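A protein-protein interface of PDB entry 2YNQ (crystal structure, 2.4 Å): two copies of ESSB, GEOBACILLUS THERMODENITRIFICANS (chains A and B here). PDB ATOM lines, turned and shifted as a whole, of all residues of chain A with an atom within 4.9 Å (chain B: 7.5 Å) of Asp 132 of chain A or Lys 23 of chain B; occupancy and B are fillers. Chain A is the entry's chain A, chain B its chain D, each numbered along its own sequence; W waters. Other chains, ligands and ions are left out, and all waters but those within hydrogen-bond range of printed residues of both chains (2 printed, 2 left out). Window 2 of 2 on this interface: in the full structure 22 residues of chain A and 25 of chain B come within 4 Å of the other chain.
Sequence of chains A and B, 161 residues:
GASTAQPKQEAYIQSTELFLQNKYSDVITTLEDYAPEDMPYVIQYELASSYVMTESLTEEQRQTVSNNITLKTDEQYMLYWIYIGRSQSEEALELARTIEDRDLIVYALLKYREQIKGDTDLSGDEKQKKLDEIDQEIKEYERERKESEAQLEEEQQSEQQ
The side-chain carboxylate of Asp 132 of chain A is in salt-bridge range of the side-chain amino group of Lys 23 of chain B (3.4 Å).
O of Gln 21 of chain B sits close to OE1 of Gln 136 of chain A, 3.5 Å away.
N of Tyr 24 of chain B lies within hydrogen-bond range of OD2 of Asp 135 of chain A, at 3.4 Å.
The side-chain amide oxygen (OE1) of Gln 136 of chain A sits at hydrogen-bond distance from the side-chain amide nitrogen (ND2) of Asn 22 of chain B (2.8 Å).
OG of Ser 25 of chain B sits at hydrogen-bond distance from OD2 of Asp 135 of chain A.
The side-chain amide nitrogen (NE2) of Gln 128 of chain A lies within hydrogen-bond range of the side-chain carboxylate (OD1) of Asp 132 of chain A.
O of Asp 26 of chain B sits at hydrogen-bond distance from OG1 of Thr 29 of chain B (3.5 Å).
O of Leu 18 of chain B lies within hydrogen-bond range of N of Lys 23 of chain B (2.9 Å).
The backbone carbonyl oxygen (O) of Asp 26 of chain B lies within hydrogen-bond range of the side-chain hydroxyl (OG1) of Thr 30 of chain B.
O of Glu 17 of chain B is in hydrogen-bond range of NE2 of Gln 21 of chain B, at 2.9 Å.
The backbone carbonyl oxygen of Ser 50 of chain B sits at hydrogen-bond distance from the side-chain hydroxyl of Thr 54 of chain B (2.9 Å).
Gln 128 of chain A touches Asp 26 of chain B (NE2 to CB, 3.6 Å).
CB of Leu 131 of chain A touches OG of Ser 25 of chain B (3.5 Å).
Asn 22 of chain B touches Asp 135 of chain A (O to CB, 3.4 Å).
Lys 23 of chain B touches Asp 135 of chain A (C to OD2, 3.9 Å).
CG2 of Thr 54 of chain B touches OD1 of Asp 135 of chain A (3.9 Å).
Of chain B, only Lys 23 comes within 4 Å of Asp 132 of chain A.
Of chain A, only Asp 132 (3.4 Å) and Asp 135 (3.9 Å) come within 4 Å of Lys 23 of chain B.
Printed residues of chain A within 4 Å of Ser 25 of chain B: Leu 131 (3.5 Å) and Asp 135 (2.6 Å).
Of the printed residues of chain B, Gln 136 of chain A touches Gln 21 (3.5 Å) and Asn 22 (2.8 Å).
Thr 29 of chain B touches none of the printed residues of chain A.
The nearest residue of chain B that does not touch Asp 132 of chain A is Asp 26 of chain B (4.4 Å).
The nearest printed residue of chain B that does not touch Gln 136 of chain A is Tyr 24 of chain B (5.4 Å).
Of the 9 printed residues of chain A, 5 touch a printed residue of chain B.
Hydrophobic or aromatic side chains of chain A that line the printed part of chain B: Leu 131.
Of the 17 printed residues of chain B, 7 touch a printed residue of chain A.
Hydrophobic or aromatic side chains of chain B within 4 Å of the printed part of chain A: Tyr 24.
Among the printed residues, 10 pairs touch across the chains.
Among the printed residues, Asp or Glu carboxylates within 4 Å of a Lys or Arg side-chain nitrogen of the other chain: Asp 132 of chain A with Lys 23 of chain B (3.4 Å).
No position is printed for both chains.
Of the 10 pairs that touch across the chains among the printed residues, none has its exchanged pair printed and touching as well.
Water W2 bridges the side-chain amide oxygen (OE1) of Gln 136 of chain A (3.2 Å) and the backbone carbonyl oxygen (O) of Gln 21 of chain B (3.5 Å).
Water W1 bridges NE2 of Gln 136 of chain A (3.3 Å) and ND2 of Asn 22 of chain B (3.3 Å).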
ATOM      1  N   GLN A 128      28.462  -9.801   0.185  1.00  0.00           N
ATOM      2  CA  GLN A 128      27.862  -8.969   1.214  1.00  0.00           C
ATOM      3  C   GLN A 128      26.353  -8.829   1.019  1.00  0.00           C
ATOM      4  O   GLN A 128      25.602  -8.927   1.986  1.00  0.00           O
ATOM      5  CB  GLN A 128      28.562  -7.602   1.304  1.00  0.00           C
ATOM      6  CG  GLN A 128      28.296  -6.799   2.604  1.00  0.00           C
ATOM      7  CD  GLN A 128      28.581  -7.585   3.900  1.00  0.00           C
ATOM      8  OE1 GLN A 128      29.733  -7.914   4.212  1.00  0.00           O
ATOM      9  NE2 GLN A 128      27.529  -7.870   4.661  1.00  0.00           N
ATOM     10  N   LYS A 129      25.902  -8.636  -0.217  1.00  0.00           N
ATOM     11  CA  LYS A 129      24.470  -8.503  -0.468  1.00  0.00           C
ATOM     12  C   LYS A 129      23.727  -9.785  -0.097  1.00  0.00           C
ATOM     13  O   LYS A 129      22.625  -9.722   0.455  1.00  0.00           O
ATOM     14  CB  LYS A 129      24.168  -8.094  -1.916  1.00  0.00           C
ATOM     15  CG  LYS A 129      22.848  -7.315  -2.055  1.00  0.00           C
ATOM     16  CD  LYS A 129      22.397  -7.141  -3.511  1.00  0.00           C
ATOM     17  CE  LYS A 129      21.494  -8.306  -3.966  1.00  0.00           C
ATOM     18  NZ  LYS A 129      20.989  -8.136  -5.357  1.00  0.00           N
ATOM     19  N   LYS A 130      24.337 -10.935  -0.395  1.00  0.00           N
ATOM     20  CA  LYS A 130      23.792 -12.248  -0.020  1.00  0.00           C
ATOM     21  C   LYS A 130      23.696 -12.455   1.506  1.00  0.00           C
ATOM     22  O   LYS A 130      22.650 -12.879   2.035  1.00  0.00           O
ATOM     23  CB  LYS A 130      24.610 -13.387  -0.659  1.00  0.00           C
ATOM     24  CG  LYS A 130      23.905 -14.137  -1.789  1.00  0.00           C
ATOM     25  CD  LYS A 130      22.783 -15.053  -1.246  1.00  0.00           C
ATOM     26  CE  LYS A 130      21.948 -15.666  -2.384  1.00  0.00           C
ATOM     27  NZ  LYS A 130      20.917 -16.617  -1.869  1.00  0.00           N
ATOM     28  N   LEU A 131      24.793 -12.160   2.200  1.00  0.00           N
ATOM     29  CA  LEU A 131      24.808 -12.196   3.650  1.00  0.00           C
ATOM     30  C   LEU A 131      23.762 -11.239   4.246  1.00  0.00           C
ATOM     31  O   LEU A 131      23.011 -11.634   5.135  1.00  0.00           O
ATOM     32  CB  LEU A 131      26.212 -11.905   4.169  1.00  0.00           C
ATOM     33  CG  LEU A 131      27.256 -12.996   3.870  1.00  0.00           C
ATOM     34  CD1 LEU A 131      28.653 -12.524   4.234  1.00  0.00           C
ATOM     35  CD2 LEU A 131      26.934 -14.299   4.586  1.00  0.00           C
ATOM     36  N   ASP A 132      23.683 -10.010   3.722  1.00  0.00           N
ATOM     37  CA  ASP A 132      22.672  -9.026   4.163  1.00  0.00           C
ATOM     38  C   ASP A 132      21.262  -9.619   4.095  1.00  0.00           C
ATOM     39  O   ASP A 132      20.465  -9.437   5.019  1.00  0.00           O
ATOM     40  CB  ASP A 132      22.728  -7.727   3.340  1.00  0.00           C
ATOM     41  CG  ASP A 132      23.914  -6.800   3.725  1.00  0.00           C
ATOM     42  OD1 ASP A 132      24.627  -7.079   4.716  1.00  0.00           O
ATOM     43  OD2 ASP A 132      24.128  -5.771   3.030  1.00  0.00           O
ATOM     44  N   GLU A 133      20.976 -10.351   3.017  1.00  0.00           N
ATOM     45  CA  GLU A 133      19.661 -10.942   2.812  1.00  0.00           C
ATOM     46  C   GLU A 133      19.405 -12.063   3.804  1.00  0.00           C
ATOM     47  O   GLU A 133      18.326 -12.127   4.401  1.00  0.00           O
ATOM     48  CB  GLU A 133      19.504 -11.471   1.381  1.00  0.00           C
ATOM     49  CG  GLU A 133      19.340 -10.398   0.306  1.00  0.00           C
ATOM     50  CD  GLU A 133      19.297 -10.988  -1.122  1.00  0.00           C
ATOM     51  OE1 GLU A 133      18.953 -12.196  -1.279  1.00  0.00           O
ATOM     52  OE2 GLU A 133      19.615 -10.238  -2.082  1.00  0.00           O
ATOM     53  N   ILE A 134      20.393 -12.943   3.975  1.00  0.00           N
ATOM     54  CA  ILE A 134      20.276 -14.048   4.922  1.00  0.00           C
ATOM     55  C   ILE A 134      20.120 -13.502   6.341  1.00  0.00           C
ATOM     56  O   ILE A 134      19.284 -13.995   7.122  1.00  0.00           O
ATOM     57  CB  ILE A 134      21.485 -15.004   4.823  1.00  0.00           C
ATOM     58  CG1 ILE A 134      21.524 -15.673   3.440  1.00  0.00           C
ATOM     59  CG2 ILE A 134      21.450 -16.053   5.916  1.00  0.00           C
ATOM     60  CD1 ILE A 134      22.793 -16.490   3.188  1.00  0.00           C
ATOM     61  N   ASP A 135      20.902 -12.469   6.662  1.00  0.00           N
ATOM     62  CA  ASP A 135      20.889 -11.902   8.004  1.00  0.00           C
ATOM     63  C   ASP A 135      19.498 -11.374   8.333  1.00  0.00           C
ATOM     64  O   ASP A 135      18.990 -11.616   9.442  1.00  0.00           O
ATOM     65  CB  ASP A 135      21.933 -10.802   8.181  1.00  0.00           C
ATOM     66  CG  ASP A 135      23.364 -11.337   8.268  1.00  0.00           C
ATOM     67  OD1 ASP A 135      23.569 -12.532   8.599  1.00  0.00           O
ATOM     68  OD2 ASP A 135      24.295 -10.541   8.008  1.00  0.00           O
ATOM     69  N   GLN A 136      18.872 -10.693   7.368  1.00  0.00           N
ATOM     70  CA  GLN A 136      17.552 -10.130   7.581  1.00  0.00           C
ATOM     71  C   GLN A 136      16.533 -11.245   7.755  1.00  0.00           C
ATOM     72  O   GLN A 136      15.713 -11.181   8.663  1.00  0.00           O
ATOM     73  CB  GLN A 136      17.156  -9.144   6.459  1.00  0.00           C
ATOM     74  CG  GLN A 136      15.739  -8.540   6.588  1.00  0.00           C
ATOM     75  CD  GLN A 136      15.562  -7.595   7.787  1.00  0.00           C
ATOM     76  OE1 GLN A 136      16.470  -6.822   8.150  1.00  0.00           O
ATOM     77  NE2 GLN A 136      14.372  -7.628   8.385  1.00  0.00           N
ATOM     78  N   SER B  15      29.037   0.402  12.858  1.00  0.00           N
ATOM     79  CA  SER B  15      28.422  -0.847  13.301  1.00  0.00           C
ATOM     80  C   SER B  15      27.015  -0.624  13.846  1.00  0.00           C
ATOM     81  O   SER B  15      26.164  -1.513  13.739  1.00  0.00           O
ATOM     82  CB  SER B  15      29.295  -1.598  14.319  1.00  0.00           C
ATOM     83  OG  SER B  15      29.320  -0.952  15.566  1.00  0.00           O
ATOM     84  N   GLU B  17      24.977   1.718  12.683  1.00  0.00           N
ATOM     85  CA  GLU B  17      24.157   1.861  11.496  1.00  0.00           C
ATOM     86  C   GLU B  17      23.780   0.505  10.874  1.00  0.00           C
ATOM     87  O   GLU B  17      22.676   0.329  10.360  1.00  0.00           O
ATOM     88  CB  GLU B  17      24.849   2.777  10.476  1.00  0.00           C
ATOM     89  CG  GLU B  17      24.157   2.847   9.122  1.00  0.00           C
ATOM     90  CD  GLU B  17      24.708   3.945   8.205  1.00  0.00           C
ATOM     91  OE1 GLU B  17      25.534   4.781   8.654  1.00  0.00           O
ATOM     92  OE2 GLU B  17      24.297   3.980   7.031  1.00  0.00           O
ATOM     93  N   LEU B  18      24.710  -0.442  10.901  1.00  0.00           N
ATOM     94  CA  LEU B  18      24.470  -1.755  10.293  1.00  0.00           C
ATOM     95  C   LEU B  18      23.612  -2.611  11.213  1.00  0.00           C
ATOM     96  O   LEU B  18      22.682  -3.274  10.753  1.00  0.00           O
ATOM     97  CB  LEU B  18      25.782  -2.455   9.951  1.00  0.00           C
ATOM     98  CG  LEU B  18      26.645  -1.737   8.908  1.00  0.00           C
ATOM     99  CD1 LEU B  18      28.071  -2.204   9.107  1.00  0.00           C
ATOM    100  CD2 LEU B  18      26.174  -1.981   7.461  1.00  0.00           C
ATOM    101  N   PHE B  19      23.880  -2.531  12.511  1.00  0.00           N
ATOM    102  CA  PHE B  19      23.116  -3.300  13.478  1.00  0.00           C
ATOM    103  C   PHE B  19      21.645  -2.941  13.520  1.00  0.00           C
ATOM    104  O   PHE B  19      20.774  -3.829  13.559  1.00  0.00           O
ATOM    105  CB  PHE B  19      23.699  -3.179  14.874  1.00  0.00           C
ATOM    106  CG  PHE B  19      22.992  -4.028  15.873  1.00  0.00           C
ATOM    107  CD1 PHE B  19      23.203  -5.419  15.891  1.00  0.00           C
ATOM    108  CD2 PHE B  19      22.098  -3.452  16.781  1.00  0.00           C
ATOM    109  CE1 PHE B  19      22.536  -6.216  16.793  1.00  0.00           C
ATOM    110  CE2 PHE B  19      21.414  -4.249  17.690  1.00  0.00           C
ATOM    111  CZ  PHE B  19      21.636  -5.637  17.705  1.00  0.00           C
ATOM    112  N   LEU B  20      21.363  -1.636  13.509  1.00  0.00           N
ATOM    113  CA  LEU B  20      19.989  -1.137  13.530  1.00  0.00           C
ATOM    114  C   LEU B  20      19.178  -1.606  12.320  1.00  0.00           C
ATOM    115  O   LEU B  20      17.952  -1.503  12.325  1.00  0.00           O
ATOM    116  CB  LEU B  20      19.988   0.385  13.632  1.00  0.00           C
ATOM    117  CG  LEU B  20      20.380   0.884  15.017  1.00  0.00           C
ATOM    118  CD1 LEU B  20      20.349   2.388  15.067  1.00  0.00           C
ATOM    119  CD2 LEU B  20      19.443   0.299  16.046  1.00  0.00           C
ATOM    120  N   GLN B  21      19.893  -2.134  11.318  1.00  0.00           N
ATOM    121  CA  GLN B  21      19.355  -2.706  10.087  1.00  0.00           C
ATOM    122  C   GLN B  21      19.455  -4.224  10.037  1.00  0.00           C
ATOM    123  O   GLN B  21      19.193  -4.818   8.975  1.00  0.00           O
ATOM    124  CB  GLN B  21      20.218  -2.257   8.916  1.00  0.00           C
ATOM    125  CG  GLN B  21      19.831  -1.003   8.302  1.00  0.00           C
ATOM    126  CD  GLN B  21      20.805  -0.607   7.223  1.00  0.00           C
ATOM    127  OE1 GLN B  21      20.561  -0.862   6.039  1.00  0.00           O
ATOM    128  NE2 GLN B  21      21.913   0.026   7.616  1.00  0.00           N
ATOM    129  N   ASN B  22      19.927  -4.835  11.130  1.00  0.00           N
ATOM    130  CA  ASN B  22      20.104  -6.295  11.221  1.00  0.00           C
ATOM    131  C   ASN B  22      21.183  -6.833  10.291  1.00  0.00           C
ATOM    132  O   ASN B  22      21.117  -7.967   9.845  1.00  0.00           O
ATOM    133  CB  ASN B  22      18.794  -7.010  10.915  1.00  0.00           C
ATOM    134  CG  ASN B  22      17.613  -6.389  11.615  1.00  0.00           C
ATOM    135  OD1 ASN B  22      17.604  -6.267  12.845  1.00  0.00           O
ATOM    136  ND2 ASN B  22      16.582  -6.012  10.838  1.00  0.00           N
ATOM    137  N   LYS B  23      22.174  -6.020   9.983  1.00  0.00           N
ATOM    138  CA  LYS B  23      23.240  -6.472   9.092  1.00  0.00           C
ATOM    139  C   LYS B  23      24.359  -7.096   9.908  1.00  0.00           C
ATOM    140  O   LYS B  23      25.466  -6.557  10.002  1.00  0.00           O
ATOM    141  CB  LYS B  23      23.744  -5.320   8.219  1.00  0.00           C
ATOM    142  CG  LYS B  23      22.777  -5.003   7.091  1.00  0.00           C
ATOM    143  CD  LYS B  23      23.282  -3.911   6.192  1.00  0.00           C
ATOM    144  CE  LYS B  23      22.285  -3.652   5.083  1.00  0.00           C
ATOM    145  NZ  LYS B  23      22.904  -2.762   4.074  1.00  0.00           N
ATOM    146  N   TYR B  24      24.045  -8.243  10.496  1.00  0.00           N
ATOM    147  CA  TYR B  24      24.934  -8.917  11.436  1.00  0.00           C
ATOM    148  C   TYR B  24      26.341  -9.174  10.870  1.00  0.00           C
ATOM    149  O   TYR B  24      27.328  -8.799  11.497  1.00  0.00           O
ATOM    150  CB  TYR B  24      24.279 -10.210  11.959  1.00  0.00           C
ATOM    151  CG  TYR B  24      22.876 -10.007  12.509  1.00  0.00           C
ATOM    152  CD1 TYR B  24      22.649  -9.151  13.573  1.00  0.00           C
ATOM    153  CD2 TYR B  24      21.779 -10.678  11.968  1.00  0.00           C
ATOM    154  CE1 TYR B  24      21.373  -8.957  14.081  1.00  0.00           C
ATOM    155  CE2 TYR B  24      20.490 -10.488  12.474  1.00  0.00           C
ATOM    156  CZ  TYR B  24      20.307  -9.621  13.537  1.00  0.00           C
ATOM    157  OH  TYR B  24      19.054  -9.395  14.066  1.00  0.00           O
ATOM    158  N   SER B  25      26.419  -9.776   9.684  1.00  0.00           N
ATOM    159  CA  SER B  25      27.702 -10.111   9.072  1.00  0.00           C
ATOM    160  C   SER B  25      28.559  -8.866   8.962  1.00  0.00           C
ATOM    161  O   SER B  25      29.748  -8.880   9.280  1.00  0.00           O
ATOM    162  CB  SER B  25      27.529 -10.733   7.677  1.00  0.00           C
ATOM    163  OG  SER B  25      26.588 -11.800   7.688  1.00  0.00           O
ATOM    164  N   ASP B  26      27.936  -7.775   8.547  1.00  0.00           N
ATOM    165  CA  ASP B  26      28.654  -6.542   8.270  1.00  0.00           C
ATOM    166  C   ASP B  26      29.099  -5.855   9.555  1.00  0.00           C
ATOM    167  O   ASP B  26      30.142  -5.194   9.573  1.00  0.00           O
ATOM    168  CB  ASP B  26      27.788  -5.624   7.409  1.00  0.00           C
ATOM    169  CG  ASP B  26      28.601  -4.781   6.446  1.00  0.00           C
ATOM    170  OD1 ASP B  26      29.849  -4.665   6.628  1.00  0.00           O
ATOM    171  OD2 ASP B  26      27.989  -4.215   5.503  1.00  0.00           O
ATOM    172  N   VAL B  27      28.315  -6.016  10.626  1.00  0.00           N
ATOM    173  CA  VAL B  27      28.706  -5.548  11.947  1.00  0.00           C
ATOM    174  C   VAL B  27      29.981  -6.250  12.366  1.00  0.00           C
ATOM    175  O   VAL B  27      30.915  -5.610  12.844  1.00  0.00           O
ATOM    176  CB  VAL B  27      27.618  -5.842  13.006  1.00  0.00           C
ATOM    177  CG1 VAL B  27      28.165  -5.662  14.417  1.00  0.00           C
ATOM    178  CG2 VAL B  27      26.392  -4.973  12.779  1.00  0.00           C
ATOM    179  N   ILE B  28      30.004  -7.569  12.158  1.00  0.00           N
ATOM    180  CA  ILE B  28      31.119  -8.433  12.520  1.00  0.00           C
ATOM    181  C   ILE B  28      32.403  -8.029  11.808  1.00  0.00           C
ATOM    182  O   ILE B  28      33.399  -7.821  12.475  1.00  0.00           O
ATOM    183  CB  ILE B  28      30.776  -9.937  12.300  1.00  0.00           C
ATOM    184  CG1 ILE B  28      29.831 -10.404  13.412  1.00  0.00           C
ATOM    185  CG2 ILE B  28      32.045 -10.829  12.242  1.00  0.00           C
ATOM    186  CD1 ILE B  28      29.017 -11.660  13.078  1.00  0.00           C
ATOM    187  N   THR B  29      32.375  -7.876  10.480  1.00  0.00           N
ATOM    188  CA  THR B  29      33.579  -7.462   9.771  1.00  0.00           C
ATOM    189  C   THR B  29      34.004  -6.024  10.067  1.00  0.00           C
ATOM    190  O   THR B  29      35.195  -5.707  10.057  1.00  0.00           O
ATOM    191  CB  THR B  29      33.511  -7.714   8.248  1.00  0.00           C
ATOM    192  OG1 THR B  29      32.389  -7.040   7.716  1.00  0.00           O
ATOM    193  CG2 THR B  29      33.368  -9.205   7.953  1.00  0.00           C
ATOM    194  N   THR B  30      33.047  -5.162  10.380  1.00  0.00           N
ATOM    195  CA  THR B  30      33.386  -3.794  10.791  1.00  0.00           C
ATOM    196  C   THR B  30      34.242  -3.784  12.055  1.00  0.00           C
ATOM    197  O   THR B  30      35.146  -2.966  12.196  1.00  0.00           O
ATOM    198  CB  THR B  30      32.115  -2.945  10.980  1.00  0.00           C
ATOM    199  OG1 THR B  30      31.479  -2.809   9.709  1.00  0.00           O
ATOM    200  CG2 THR B  30      32.433  -1.548  11.531  1.00  0.00           C
ATOM    201  N   SER B  50      25.186  -9.898  17.258  1.00  0.00           N
ATOM    202  CA  SER B  50      25.424 -10.262  15.873  1.00  0.00           C
ATOM    203  C   SER B  50      26.027 -11.665  15.794  1.00  0.00           C
ATOM    204  O   SER B  50      25.600 -12.464  14.957  1.00  0.00           O
ATOM    205  CB  SER B  50      26.289  -9.236  15.160  1.00  0.00           C
ATOM    206  OG  SER B  50      25.614  -7.992  15.091  1.00  0.00           O
ATOM    207  N   THR B  54      23.984 -15.361  14.506  1.00  0.00           N
ATOM    208  CA  THR B  54      24.517 -16.061  13.347  1.00  0.00           C
ATOM    209  C   THR B  54      25.275 -17.334  13.748  1.00  0.00           C
ATOM    210  O   THR B  54      25.960 -17.938  12.926  1.00  0.00           O
ATOM    211  CB  THR B  54      25.451 -15.135  12.534  1.00  0.00           C
ATOM    212  OG1 THR B  54      26.509 -14.656  13.376  1.00  0.00           O
ATOM    213  CG2 THR B  54      24.692 -13.950  12.006  1.00  0.00           C
HETATM  214  O   HOH W   1      13.311  -5.657  10.775  1.00  0.00           O
HETATM  215  O   HOH W   2      16.145  -3.677   7.785  1.00  0.00           O
